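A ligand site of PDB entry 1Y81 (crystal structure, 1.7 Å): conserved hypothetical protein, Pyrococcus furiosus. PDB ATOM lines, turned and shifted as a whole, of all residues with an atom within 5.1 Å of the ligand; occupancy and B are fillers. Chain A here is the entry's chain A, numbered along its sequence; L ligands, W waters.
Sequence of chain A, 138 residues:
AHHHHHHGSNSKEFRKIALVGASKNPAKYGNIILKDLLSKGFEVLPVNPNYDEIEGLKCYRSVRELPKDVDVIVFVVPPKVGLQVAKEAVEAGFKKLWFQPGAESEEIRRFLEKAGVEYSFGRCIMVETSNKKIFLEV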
ATOM      1  N   VAL A  20     -30.929  30.188 -11.121  1.00  0.00           N
ATOM      2  CA  VAL A  20     -29.485  30.351 -10.941  1.00  0.00           C
ATOM      3  C   VAL A  20     -28.832  30.134 -12.321  1.00  0.00           C
ATOM      4  O   VAL A  20     -28.958  29.056 -12.895  1.00  0.00           O
ATOM      5  CB  VAL A  20     -28.904  29.359  -9.897  1.00  0.00           C
ATOM      6  CG1 VAL A  20     -27.343  29.387  -9.900  1.00  0.00           C
ATOM      7  CG2 VAL A  20     -29.461  29.646  -8.475  1.00  0.00           C
ATOM      8  N   GLY A  21     -28.154  31.158 -12.829  1.00  0.00           N
ATOM      9  CA  GLY A  21     -27.625  31.149 -14.188  1.00  0.00           C
ATOM     10  C   GLY A  21     -28.505  31.861 -15.196  1.00  0.00           C
ATOM     11  O   GLY A  21     -28.223  31.812 -16.403  1.00  0.00           O
ATOM     12  N   ALA A  22     -29.556  32.544 -14.720  1.00  0.00           N
ATOM     13  CA  ALA A  22     -30.345  33.413 -15.588  1.00  0.00           C
ATOM     14  C   ALA A  22     -29.392  34.356 -16.303  1.00  0.00           C
ATOM     15  O   ALA A  22     -28.419  34.771 -15.728  1.00  0.00           O
ATOM     16  CB  ALA A  22     -31.344  34.236 -14.774  1.00  0.00           C
ATOM     17  N   SER A  23     -29.687  34.669 -17.568  1.00  0.00           N
ATOM     18  CA  SER A  23     -28.771  35.459 -18.371  1.00  0.00           C
ATOM     19  C   SER A  23     -29.524  36.418 -19.267  1.00  0.00           C
ATOM     20  O   SER A  23     -30.688  36.189 -19.573  1.00  0.00           O
ATOM     21  CB  SER A  23     -27.929  34.532 -19.252  1.00  0.00           C
ATOM     22  OG  SER A  23     -27.056  35.295 -20.051  1.00  0.00           O
ATOM     23  N   ASN A  25     -28.142  36.986 -22.191  1.00  0.00           N
ATOM     24  CA  ASN A  25     -27.749  36.431 -23.483  1.00  0.00           C
ATOM     25  C   ASN A  25     -28.849  35.540 -24.062  1.00  0.00           C
ATOM     26  O   ASN A  25     -29.111  34.458 -23.529  1.00  0.00           O
ATOM     27  CB  ASN A  25     -26.422  35.644 -23.333  1.00  0.00           C
ATOM     28  CG  ASN A  25     -25.903  35.101 -24.672  1.00  0.00           C
ATOM     29  OD1 ASN A  25     -26.621  35.082 -25.699  1.00  0.00           O
ATOM     30  ND2 ASN A  25     -24.656  34.627 -24.664  1.00  0.00           N
ATOM     31  N   LYS A  28     -28.518  31.748 -24.450  1.00  0.00           N
ATOM     32  CA  LYS A  28     -28.272  30.900 -23.297  1.00  0.00           C
ATOM     33  C   LYS A  28     -29.580  30.428 -22.676  1.00  0.00           C
ATOM     34  O   LYS A  28     -30.564  31.179 -22.627  1.00  0.00           O
ATOM     35  CB  LYS A  28     -27.412  31.636 -22.265  1.00  0.00           C
ATOM     36  CG  LYS A  28     -25.922  31.819 -22.663  1.00  0.00           C
ATOM     37  CD  LYS A  28     -25.074  30.610 -22.178  1.00  0.00           C
ATOM     38  CE  LYS A  28     -23.569  30.838 -22.337  1.00  0.00           C
ATOM     39  NZ  LYS A  28     -23.127  32.182 -21.856  1.00  0.00           N
ATOM     40  N   TYR A  29     -29.588  29.198 -22.185  1.00  0.00           N
ATOM     41  CA  TYR A  29     -30.787  28.660 -21.505  1.00  0.00           C
ATOM     42  C   TYR A  29     -31.235  29.511 -20.290  1.00  0.00           C
ATOM     43  O   TYR A  29     -32.410  29.560 -19.966  1.00  0.00           O
ATOM     44  CB  TYR A  29     -30.599  27.190 -21.144  1.00  0.00           C
ATOM     45  CG  TYR A  29     -30.973  26.271 -22.305  1.00  0.00           C
ATOM     46  CD1 TYR A  29     -32.294  26.185 -22.734  1.00  0.00           C
ATOM     47  CD2 TYR A  29     -29.989  25.534 -23.011  1.00  0.00           C
ATOM     48  CE1 TYR A  29     -32.668  25.355 -23.810  1.00  0.00           C
ATOM     49  CE2 TYR A  29     -30.359  24.689 -24.103  1.00  0.00           C
ATOM     50  CZ  TYR A  29     -31.696  24.624 -24.481  1.00  0.00           C
ATOM     51  OH  TYR A  29     -32.108  23.815 -25.529  1.00  0.00           O
ATOM     52  N   ILE A  33     -35.124  30.024 -20.643  1.00  0.00           N
ATOM     53  CA  ILE A  33     -35.960  29.519 -19.544  1.00  0.00           C
ATOM     54  C   ILE A  33     -36.694  30.671 -18.857  1.00  0.00           C
ATOM     55  O   ILE A  33     -37.914  30.600 -18.647  1.00  0.00           O
ATOM     56  CB  ILE A  33     -35.129  28.696 -18.536  1.00  0.00           C
ATOM     57  CG1 ILE A  33     -34.575  27.429 -19.230  1.00  0.00           C
ATOM     58  CG2 ILE A  33     -35.976  28.318 -17.280  1.00  0.00           C
ATOM     59  CD1 ILE A  33     -33.475  26.774 -18.439  1.00  0.00           C
ATOM     60  N   VAL A  47     -30.972  34.898 -10.816  1.00  0.00           N
ATOM     61  CA  VAL A  47     -29.829  34.937  -9.935  1.00  0.00           C
ATOM     62  C   VAL A  47     -28.549  34.812 -10.778  1.00  0.00           C
ATOM     63  O   VAL A  47     -28.277  33.764 -11.388  1.00  0.00           O
ATOM     64  CB  VAL A  47     -29.883  33.808  -8.854  1.00  0.00           C
ATOM     65  CG1 VAL A  47     -28.613  33.808  -8.014  1.00  0.00           C
ATOM     66  CG2 VAL A  47     -31.223  33.894  -7.993  1.00  0.00           C
ATOM     67  N   ASN A  48     -27.777  35.896 -10.814  1.00  0.00           N
ATOM     68  CA  ASN A  48     -26.537  35.970 -11.610  1.00  0.00           C
ATOM     69  C   ASN A  48     -25.802  37.268 -11.229  1.00  0.00           C
ATOM     70  O   ASN A  48     -26.335  38.342 -11.436  1.00  0.00           O
ATOM     71  CB  ASN A  48     -26.828  35.916 -13.120  1.00  0.00           C
ATOM     72  CG  ASN A  48     -25.524  35.863 -13.982  1.00  0.00           C
ATOM     73  OD1 ASN A  48     -24.475  36.368 -13.592  1.00  0.00           O
ATOM     74  ND2 ASN A  48     -25.614  35.224 -15.138  1.00  0.00           N
ATOM     75  N   PRO A  49     -24.583  37.158 -10.650  1.00  0.00           N
ATOM     76  CA  PRO A  49     -23.773  38.340 -10.244  1.00  0.00           C
ATOM     77  C   PRO A  49     -23.429  39.316 -11.379  1.00  0.00           C
ATOM     78  O   PRO A  49     -23.099  40.476 -11.104  1.00  0.00           O
ATOM     79  CB  PRO A  49     -22.471  37.727  -9.691  1.00  0.00           C
ATOM     80  CG  PRO A  49     -22.765  36.287  -9.449  1.00  0.00           C
ATOM     81  CD  PRO A  49     -23.901  35.877 -10.349  1.00  0.00           C
ATOM     82  N   ASN A  50     -23.519  38.868 -12.640  1.00  0.00           N
ATOM     83  CA  ASN A  50     -23.189  39.727 -13.805  1.00  0.00           C
ATOM     84  C   ASN A  50     -24.223  40.810 -14.127  1.00  0.00           C
ATOM     85  O   ASN A  50     -23.896  41.810 -14.812  1.00  0.00           O
ATOM     86  CB  ASN A  50     -23.018  38.874 -15.091  1.00  0.00           C
ATOM     87  CG  ASN A  50     -21.723  38.086 -15.119  1.00  0.00           C
ATOM     88  OD1 ASN A  50     -21.613  37.097 -15.856  1.00  0.00           O
ATOM     89  ND2 ASN A  50     -20.735  38.493 -14.335  1.00  0.00           N
ATOM     90  N   TYR A  51     -25.471  40.608 -13.690  1.00  0.00           N
ATOM     91  CA  TYR A  51     -26.589  41.466 -14.104  1.00  0.00           C
ATOM     92  C   TYR A  51     -27.289  42.054 -12.913  1.00  0.00           C
ATOM     93  O   TYR A  51     -27.503  41.358 -11.919  1.00  0.00           O
ATOM     94  CB  TYR A  51     -27.573  40.688 -14.999  1.00  0.00           C
ATOM     95  CG  TYR A  51     -26.873  39.944 -16.106  1.00  0.00           C
ATOM     96  CD1 TYR A  51     -26.221  40.645 -17.123  1.00  0.00           C
ATOM     97  CD2 TYR A  51     -26.842  38.543 -16.135  1.00  0.00           C
ATOM     98  CE1 TYR A  51     -25.552  39.981 -18.132  1.00  0.00           C
ATOM     99  CE2 TYR A  51     -26.170  37.857 -17.153  1.00  0.00           C
ATOM    100  CZ  TYR A  51     -25.518  38.589 -18.150  1.00  0.00           C
ATOM    101  OH  TYR A  51     -24.845  37.970 -19.168  1.00  0.00           O
ATOM    102  N   ARG A  61     -27.519  38.672  -6.669  1.00  0.00           N
ATOM    103  CA  ARG A  61     -26.105  38.264  -6.743  1.00  0.00           C
ATOM    104  C   ARG A  61     -25.927  36.810  -6.337  1.00  0.00           C
ATOM    105  O   ARG A  61     -25.111  36.090  -6.929  1.00  0.00           O
ATOM    106  CB  ARG A  61     -25.196  39.158  -5.873  1.00  0.00           C
ATOM    107  CG  ARG A  61     -25.063  40.581  -6.375  1.00  0.00           C
ATOM    108  N   VAL A  76     -29.074  26.362 -13.885  1.00  0.00           N
ATOM    109  CA  VAL A  76     -28.588  26.207 -15.252  1.00  0.00           C
ATOM    110  C   VAL A  76     -27.115  26.725 -15.367  1.00  0.00           C
ATOM    111  O   VAL A  76     -26.745  27.489 -16.292  1.00  0.00           O
ATOM    112  CB  VAL A  76     -29.596  26.835 -16.264  1.00  0.00           C
ATOM    113  CG1 VAL A  76     -29.613  28.351 -16.148  1.00  0.00           C
ATOM    114  CG2 VAL A  76     -29.314  26.374 -17.706  1.00  0.00           C
ATOM    115  N   VAL A  77     -26.279  26.293 -14.407  1.00  0.00           N
ATOM    116  CA  VAL A  77     -24.863  26.622 -14.351  1.00  0.00           C
ATOM    117  C   VAL A  77     -24.041  25.307 -14.360  1.00  0.00           C
ATOM    118  O   VAL A  77     -24.598  24.254 -14.021  1.00  0.00           O
ATOM    119  CB  VAL A  77     -24.494  27.452 -13.078  1.00  0.00           C
ATOM    120  CG1 VAL A  77     -25.180  28.791 -13.100  1.00  0.00           C
ATOM    121  CG2 VAL A  77     -24.884  26.699 -11.764  1.00  0.00           C
ATOM    122  N   PRO A  78     -22.737  25.375 -14.734  1.00  0.00           N
ATOM    123  CA  PRO A  78     -21.881  24.172 -14.685  1.00  0.00           C
ATOM    124  C   PRO A  78     -21.858  23.558 -13.277  1.00  0.00           C
ATOM    125  O   PRO A  78     -21.976  24.284 -12.289  1.00  0.00           O
ATOM    126  CB  PRO A  78     -20.497  24.700 -15.070  1.00  0.00           C
ATOM    127  CG  PRO A  78     -20.753  25.940 -15.830  1.00  0.00           C
ATOM    128  CD  PRO A  78     -21.979  26.551 -15.219  1.00  0.00           C
ATOM    129  N   PRO A  79     -21.732  22.211 -13.175  1.00  0.00           N
ATOM    130  CA  PRO A  79     -21.806  21.508 -11.878  1.00  0.00           C
ATOM    131  C   PRO A  79     -20.830  21.995 -10.793  1.00  0.00           C
ATOM    132  O   PRO A  79     -21.177  21.956  -9.610  1.00  0.00           O
ATOM    133  CB  PRO A  79     -21.531  20.022 -12.233  1.00  0.00           C
ATOM    134  CG  PRO A  79     -21.220  19.991 -13.686  1.00  0.00           C
ATOM    135  CD  PRO A  79     -21.591  21.287 -14.320  1.00  0.00           C
ATOM    136  N   VAL A  81     -19.875  25.073 -10.306  1.00  0.00           N
ATOM    137  CA  VAL A  81     -20.590  26.255  -9.779  1.00  0.00           C
ATOM    138  C   VAL A  81     -21.827  25.826  -8.985  1.00  0.00           C
ATOM    139  O   VAL A  81     -22.086  26.346  -7.897  1.00  0.00           O
ATOM    140  CB  VAL A  81     -20.996  27.225 -10.926  1.00  0.00           C
ATOM    141  CG1 VAL A  81     -21.847  28.412 -10.383  1.00  0.00           C
ATOM    142  CG2 VAL A  81     -19.783  27.729 -11.627  1.00  0.00           C
ATOM    143  N   VAL A  85     -23.224  26.785  -5.075  1.00  0.00           N
ATOM    144  CA  VAL A  85     -24.517  27.456  -4.949  1.00  0.00           C
ATOM    145  C   VAL A  85     -25.535  26.602  -4.182  1.00  0.00           C
ATOM    146  O   VAL A  85     -26.318  27.140  -3.390  1.00  0.00           O
ATOM    147  CB  VAL A  85     -25.064  27.906  -6.322  1.00  0.00           C
ATOM    148  CG1 VAL A  85     -26.453  28.540  -6.200  1.00  0.00           C
ATOM    149  CG2 VAL A  85     -24.073  28.879  -6.977  1.00  0.00           C
ATOM    150  N   GLN A 100     -31.216  21.516 -14.205  1.00  0.00           N
ATOM    151  CA  GLN A 100     -31.384  21.239 -15.629  1.00  0.00           C
ATOM    152  C   GLN A 100     -30.326  20.243 -16.059  1.00  0.00           C
ATOM    153  O   GLN A 100     -29.238  20.226 -15.483  1.00  0.00           O
ATOM    154  CB  GLN A 100     -31.247  22.518 -16.460  1.00  0.00           C
ATOM    155  CG  GLN A 100     -32.422  23.438 -16.344  1.00  0.00           C
ATOM    156  CD  GLN A 100     -33.678  22.875 -16.958  1.00  0.00           C
ATOM    157  OE1 GLN A 100     -34.513  22.309 -16.248  1.00  0.00           O
ATOM    158  NE2 GLN A 100     -33.824  23.020 -18.283  1.00  0.00           N
ATOM    159  N   PRO A 101     -30.665  19.371 -17.051  1.00  0.00           N
ATOM    160  CA  PRO A 101     -29.650  18.444 -17.566  1.00  0.00           C
ATOM    161  C   PRO A 101     -28.370  19.177 -17.961  1.00  0.00           C
ATOM    162  O   PRO A 101     -28.430  20.173 -18.717  1.00  0.00           O
ATOM    163  CB  PRO A 101     -30.331  17.828 -18.784  1.00  0.00           C
ATOM    164  CG  PRO A 101     -31.767  17.848 -18.465  1.00  0.00           C
ATOM    165  CD  PRO A 101     -31.960  19.163 -17.702  1.00  0.00           C
ATOM    166  N   GLY A 102     -27.248  18.693 -17.430  1.00  0.00           N
ATOM    167  CA  GLY A 102     -25.932  19.294 -17.675  1.00  0.00           C
ATOM    168  C   GLY A 102     -25.386  20.017 -16.462  1.00  0.00           C
ATOM    169  O   GLY A 102     -24.181  20.250 -16.355  1.00  0.00           O
ATOM    170  N   ALA A 103     -26.294  20.357 -15.542  1.00  0.00           N
ATOM    171  CA  ALA A 103     -25.972  21.080 -14.310  1.00  0.00           C
ATOM    172  C   ALA A 103     -25.745  20.119 -13.122  1.00  0.00           C
ATOM    173  O   ALA A 103     -25.200  20.508 -12.087  1.00  0.00           O
ATOM    174  CB  ALA A 103     -27.096  22.079 -13.971  1.00  0.00           C
ATOM    175  N   ARG A 123     -34.467  16.170 -15.627  1.00  0.00           N
ATOM    176  CA  ARG A 123     -35.782  16.634 -16.061  1.00  0.00           C
ATOM    177  C   ARG A 123     -35.703  18.071 -16.544  1.00  0.00           C
ATOM    178  O   ARG A 123     -35.035  18.916 -15.928  1.00  0.00           O
ATOM    179  CB  ARG A 123     -36.805  16.533 -14.934  1.00  0.00           C
ATOM    180  CG  ARG A 123     -37.240  15.104 -14.577  1.00  0.00           C
ATOM    181  CD  ARG A 123     -38.559  15.099 -13.813  1.00  0.00           C
ATOM    182  NE  ARG A 123     -38.406  15.590 -12.443  1.00  0.00           N
ATOM    183  CZ  ARG A 123     -39.400  16.103 -11.716  1.00  0.00           C
ATOM    184  NH1 ARG A 123     -40.639  16.213 -12.225  1.00  0.00           N
ATOM    185  NH2 ARG A 123     -39.173  16.516 -10.474  1.00  0.00           N
ATOM    186  N   CYS A 124     -36.394  18.328 -17.650  1.00  0.00           N
ATOM    187  CA  CYS A 124     -36.388  19.620 -18.286  1.00  0.00           C
ATOM    188  C   CYS A 124     -37.532  20.524 -17.751  1.00  0.00           C
ATOM    189  O   CYS A 124     -38.687  20.238 -17.983  1.00  0.00           O
ATOM    190  CB  CYS A 124     -36.550  19.405 -19.791  1.00  0.00           C
ATOM    191  SG  CYS A 124     -35.146  18.576 -20.557  1.00  0.00           S
ATOM    192  N   MET A 126     -38.879  23.429 -18.664  1.00  0.00           N
ATOM    193  CA  MET A 126     -39.876  23.947 -19.615  1.00  0.00           C
ATOM    194  C   MET A 126     -40.838  22.832 -20.091  1.00  0.00           C
ATOM    195  O   MET A 126     -42.012  23.075 -20.295  1.00  0.00           O
ATOM    196  CB  MET A 126     -39.243  24.673 -20.808  1.00  0.00           C
ATOM    197  CG  MET A 126     -38.282  25.789 -20.407  1.00  0.00           C
ATOM    198  SD  MET A 126     -37.685  26.845 -21.954  1.00  0.00           S
ATOM    199  CE  MET A 126     -36.138  25.814 -22.637  1.00  0.00           C
HETATM  200  N1  LIG L   1     -24.447  32.272  -9.723  1.00  0.00           N
HETATM  201  C1  LIG L   1     -25.330  32.568 -10.727  1.00  0.00           C
HETATM  202  N2  LIG L   1     -24.952  32.473 -12.038  1.00  0.00           N
HETATM  203  C2  LIG L   1     -23.675  32.116 -12.349  1.00  0.00           C
HETATM  204  C3  LIG L   1     -22.753  31.801 -11.357  1.00  0.00           C
HETATM  205  C4  LIG L   1     -23.150  31.877 -10.026  1.00  0.00           C
HETATM  206  N3  LIG L   1     -22.284  31.602  -9.064  1.00  0.00           N
HETATM  207  N4  LIG L   1     -21.588  31.453 -11.960  1.00  0.00           N
HETATM  208  C5  LIG L   1     -21.772  31.533 -13.307  1.00  0.00           C
HETATM  209  N5  LIG L   1     -23.052  31.941 -13.552  1.00  0.00           N
HETATM  210  C6  LIG L   1     -23.698  32.218 -14.852  1.00  0.00           C
HETATM  211  C7  LIG L   1     -22.697  32.437 -15.989  1.00  0.00           C
HETATM  212  O1  LIG L   1     -21.938  33.669 -15.876  1.00  0.00           O
HETATM  213  C8  LIG L   1     -23.672  32.329 -17.167  1.00  0.00           C
HETATM  214  O2  LIG L   1     -24.363  33.537 -17.415  1.00  0.00           O
HETATM  215  P1  LIG L   1     -23.757  34.662 -18.423  1.00  0.00           P
HETATM  216  O3  LIG L   1     -23.875  36.025 -17.801  1.00  0.00           O
HETATM  217  O4  LIG L   1     -24.554  34.571 -19.673  1.00  0.00           O
HETATM  218  O5  LIG L   1     -22.293  34.411 -18.583  1.00  0.00           O
HETATM  219  C9  LIG L   1     -24.707  31.302 -16.720  1.00  0.00           C
HETATM  220  O6  LIG L   1     -24.579  31.197 -15.294  1.00  0.00           O
HETATM  221  C10 LIG L   1     -24.530  29.917 -17.383  1.00  0.00           C
HETATM  222  O7  LIG L   1     -23.220  29.476 -17.107  1.00  0.00           O
HETATM  223  P2  LIG L   1     -22.224  29.037 -18.299  1.00  0.00           P
HETATM  224  O8  LIG L   1     -20.838  28.806 -17.738  1.00  0.00           O
HETATM  225  O9  LIG L   1     -22.294  30.044 -19.428  1.00  0.00           O
HETATM  226  O10 LIG L   1     -22.872  27.616 -18.689  1.00  0.00           O
HETATM  227  P3  LIG L   1     -23.586  27.273 -20.081  1.00  0.00           P
HETATM  228  O11 LIG L   1     -22.567  27.292 -21.195  1.00  0.00           O
HETATM  229  O12 LIG L   1     -24.770  28.095 -20.414  1.00  0.00           O
HETATM  230  O13 LIG L   1     -24.089  25.777 -19.832  1.00  0.00           O
HETATM  231  C11 LIG L   1     -25.048  23.974 -18.562  1.00  0.00           C
HETATM  232  C12 LIG L   1     -25.065  25.487 -18.846  1.00  0.00           C
HETATM  233  C13 LIG L   1     -26.098  23.706 -17.477  1.00  0.00           C
HETATM  234  C14 LIG L   1     -23.677  23.559 -18.013  1.00  0.00           C
HETATM  235  C15 LIG L   1     -25.325  23.170 -19.859  1.00  0.00           C
HETATM  236  O14 LIG L   1     -25.201  21.775 -19.613  1.00  0.00           O
HETATM  237  C16 LIG L   1     -26.733  23.511 -20.272  1.00  0.00           C
HETATM  238  O15 LIG L   1     -26.920  24.560 -21.168  1.00  0.00           O
HETATM  239  N6  LIG L   1     -27.711  22.809 -19.689  1.00  0.00           N
HETATM  240  C17 LIG L   1     -29.135  23.038 -19.866  1.00  0.00           C
HETATM  241  C18 LIG L   1     -29.702  22.477 -21.115  1.00  0.00           C
HETATM  242  C19 LIG L   1     -31.184  22.726 -21.100  1.00  0.00           C
HETATM  243  O16 LIG L   1     -31.741  23.511 -20.293  1.00  0.00           O
HETATM  244  N7  LIG L   1     -31.783  22.038 -22.041  1.00  0.00           N
HETATM  245  C20 LIG L   1     -33.179  22.023 -22.318  1.00  0.00           C
HETATM  246  C21 LIG L   1     -33.702  20.584 -22.299  1.00  0.00           C
HETATM  247  S1  LIG L   1     -33.560  19.873 -20.620  1.00  0.00           S
HETATM  248  O   HOH W   1     -26.524  24.204 -23.854  1.00  0.00           O
HETATM  249  O   HOH W   2     -19.991  29.921 -15.366  1.00  0.00           O
HETATM  250  O   HOH W   3     -22.114  34.942 -13.399  1.00  0.00           O
HETATM  251  O   HOH W   4     -24.944  33.204  -7.330  1.00  0.00           O
HETATM  252  O   HOH W   5     -20.910  32.312 -19.654  1.00  0.00           O
HETATM  253  O   HOH W   6     -27.574  30.637 -18.895  1.00  0.00           O
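A sulfur (S1) of the ligand is bonded to the side-chain sulfur (SG) of Cys 124, at 2.0 Å. OH of Tyr 51 is in hydrogen-bond range of O3 of the ligand, at 2.6 Å. OG of Ser 23 lies within hydrogen-bond range of O4 of the ligand. The backbone carbonyl oxygen of Pro 101 sits at hydrogen-bond distance from a nitrogen (N6) of the ligand, 2.9 Å away. The side-chain amide nitrogen of Gln 100 lies within hydrogen-bond range of an oxygen (O16) of the ligand, at 2.9 Å. NZ of Lys 28 is in salt-bridge range of O9 of the ligand, 3.3 Å away. An oxygen (O2) of the ligand lies within hydrogen-bond range of the side-chain amide nitrogen (ND2) of Asn 48, 3.1 Å away. OD1 of Asn 50 lies close to O3 of the ligand (3.2 Å).
OG of Ser 23 is in hydrogen-bond range of N of Asn 25. OE1 of Gln 100 lies close to O of Arg 123, at 3.4 Å. The backbone NH (N) of Asn 50 is in hydrogen-bond range of the side-chain amide oxygen (OD1) of Asn 48. The side-chain amide nitrogen (ND2) of Asn 48 is in hydrogen-bond range of the backbone carbonyl oxygen (O) of Ala 22 (2.9 Å). N of Gly 21 sits at hydrogen-bond distance from O of Val 47 (3.0 Å). The backbone NH of Val 76 lies within hydrogen-bond range of the backbone carbonyl oxygen of Val 20 (2.9 Å).
Val 20 touches the ligand. Gly 21 touches the ligand. CG of Tyr 29 touches O16 of the ligand, 3.5 Å away. Val 47 touches the ligand. Pro 49 touches the ligand (CD to C1, 3.6 Å). O of Val 76 touches C10 of the ligand, 3.5 Å away. CG1 of Val 77 touches O6 of the ligand (3.3 Å). Pro 78 touches the ligand. CG1 of Val 81 touches N4 of the ligand, 3.4 Å away. CG2 of Val 85 touches N3 of the ligand, at 3.9 Å. CA of Gly 102 touches O14 of the ligand, at 3.2 Å. Ala 103 touches the ligand. Hydrophobic or aromatic side chains within 4 Å of the ligand: Val 20, Tyr 29, Pro 49, Tyr 51, Val 76, Val 77, Pro 78, Val 81, Val 85, Pro 101 and Ala 103.
Water W4 bridges N1 of the ligand (2.6 Å) and O of Arg 61 (2.9 Å). Water W5 lies within hydrogen-bond range of an oxygen (O9) of the ligand (2.7 Å) and the side-chain amino group of Lys 28 (3.1 Å). Water W3 lies within hydrogen-bond range of the side-chain amide oxygen of Asn 48 (2.8 Å), an oxygen (O1) of the ligand (2.8 Å) and the side-chain amide oxygen of Asn 50 (3.3 Å).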
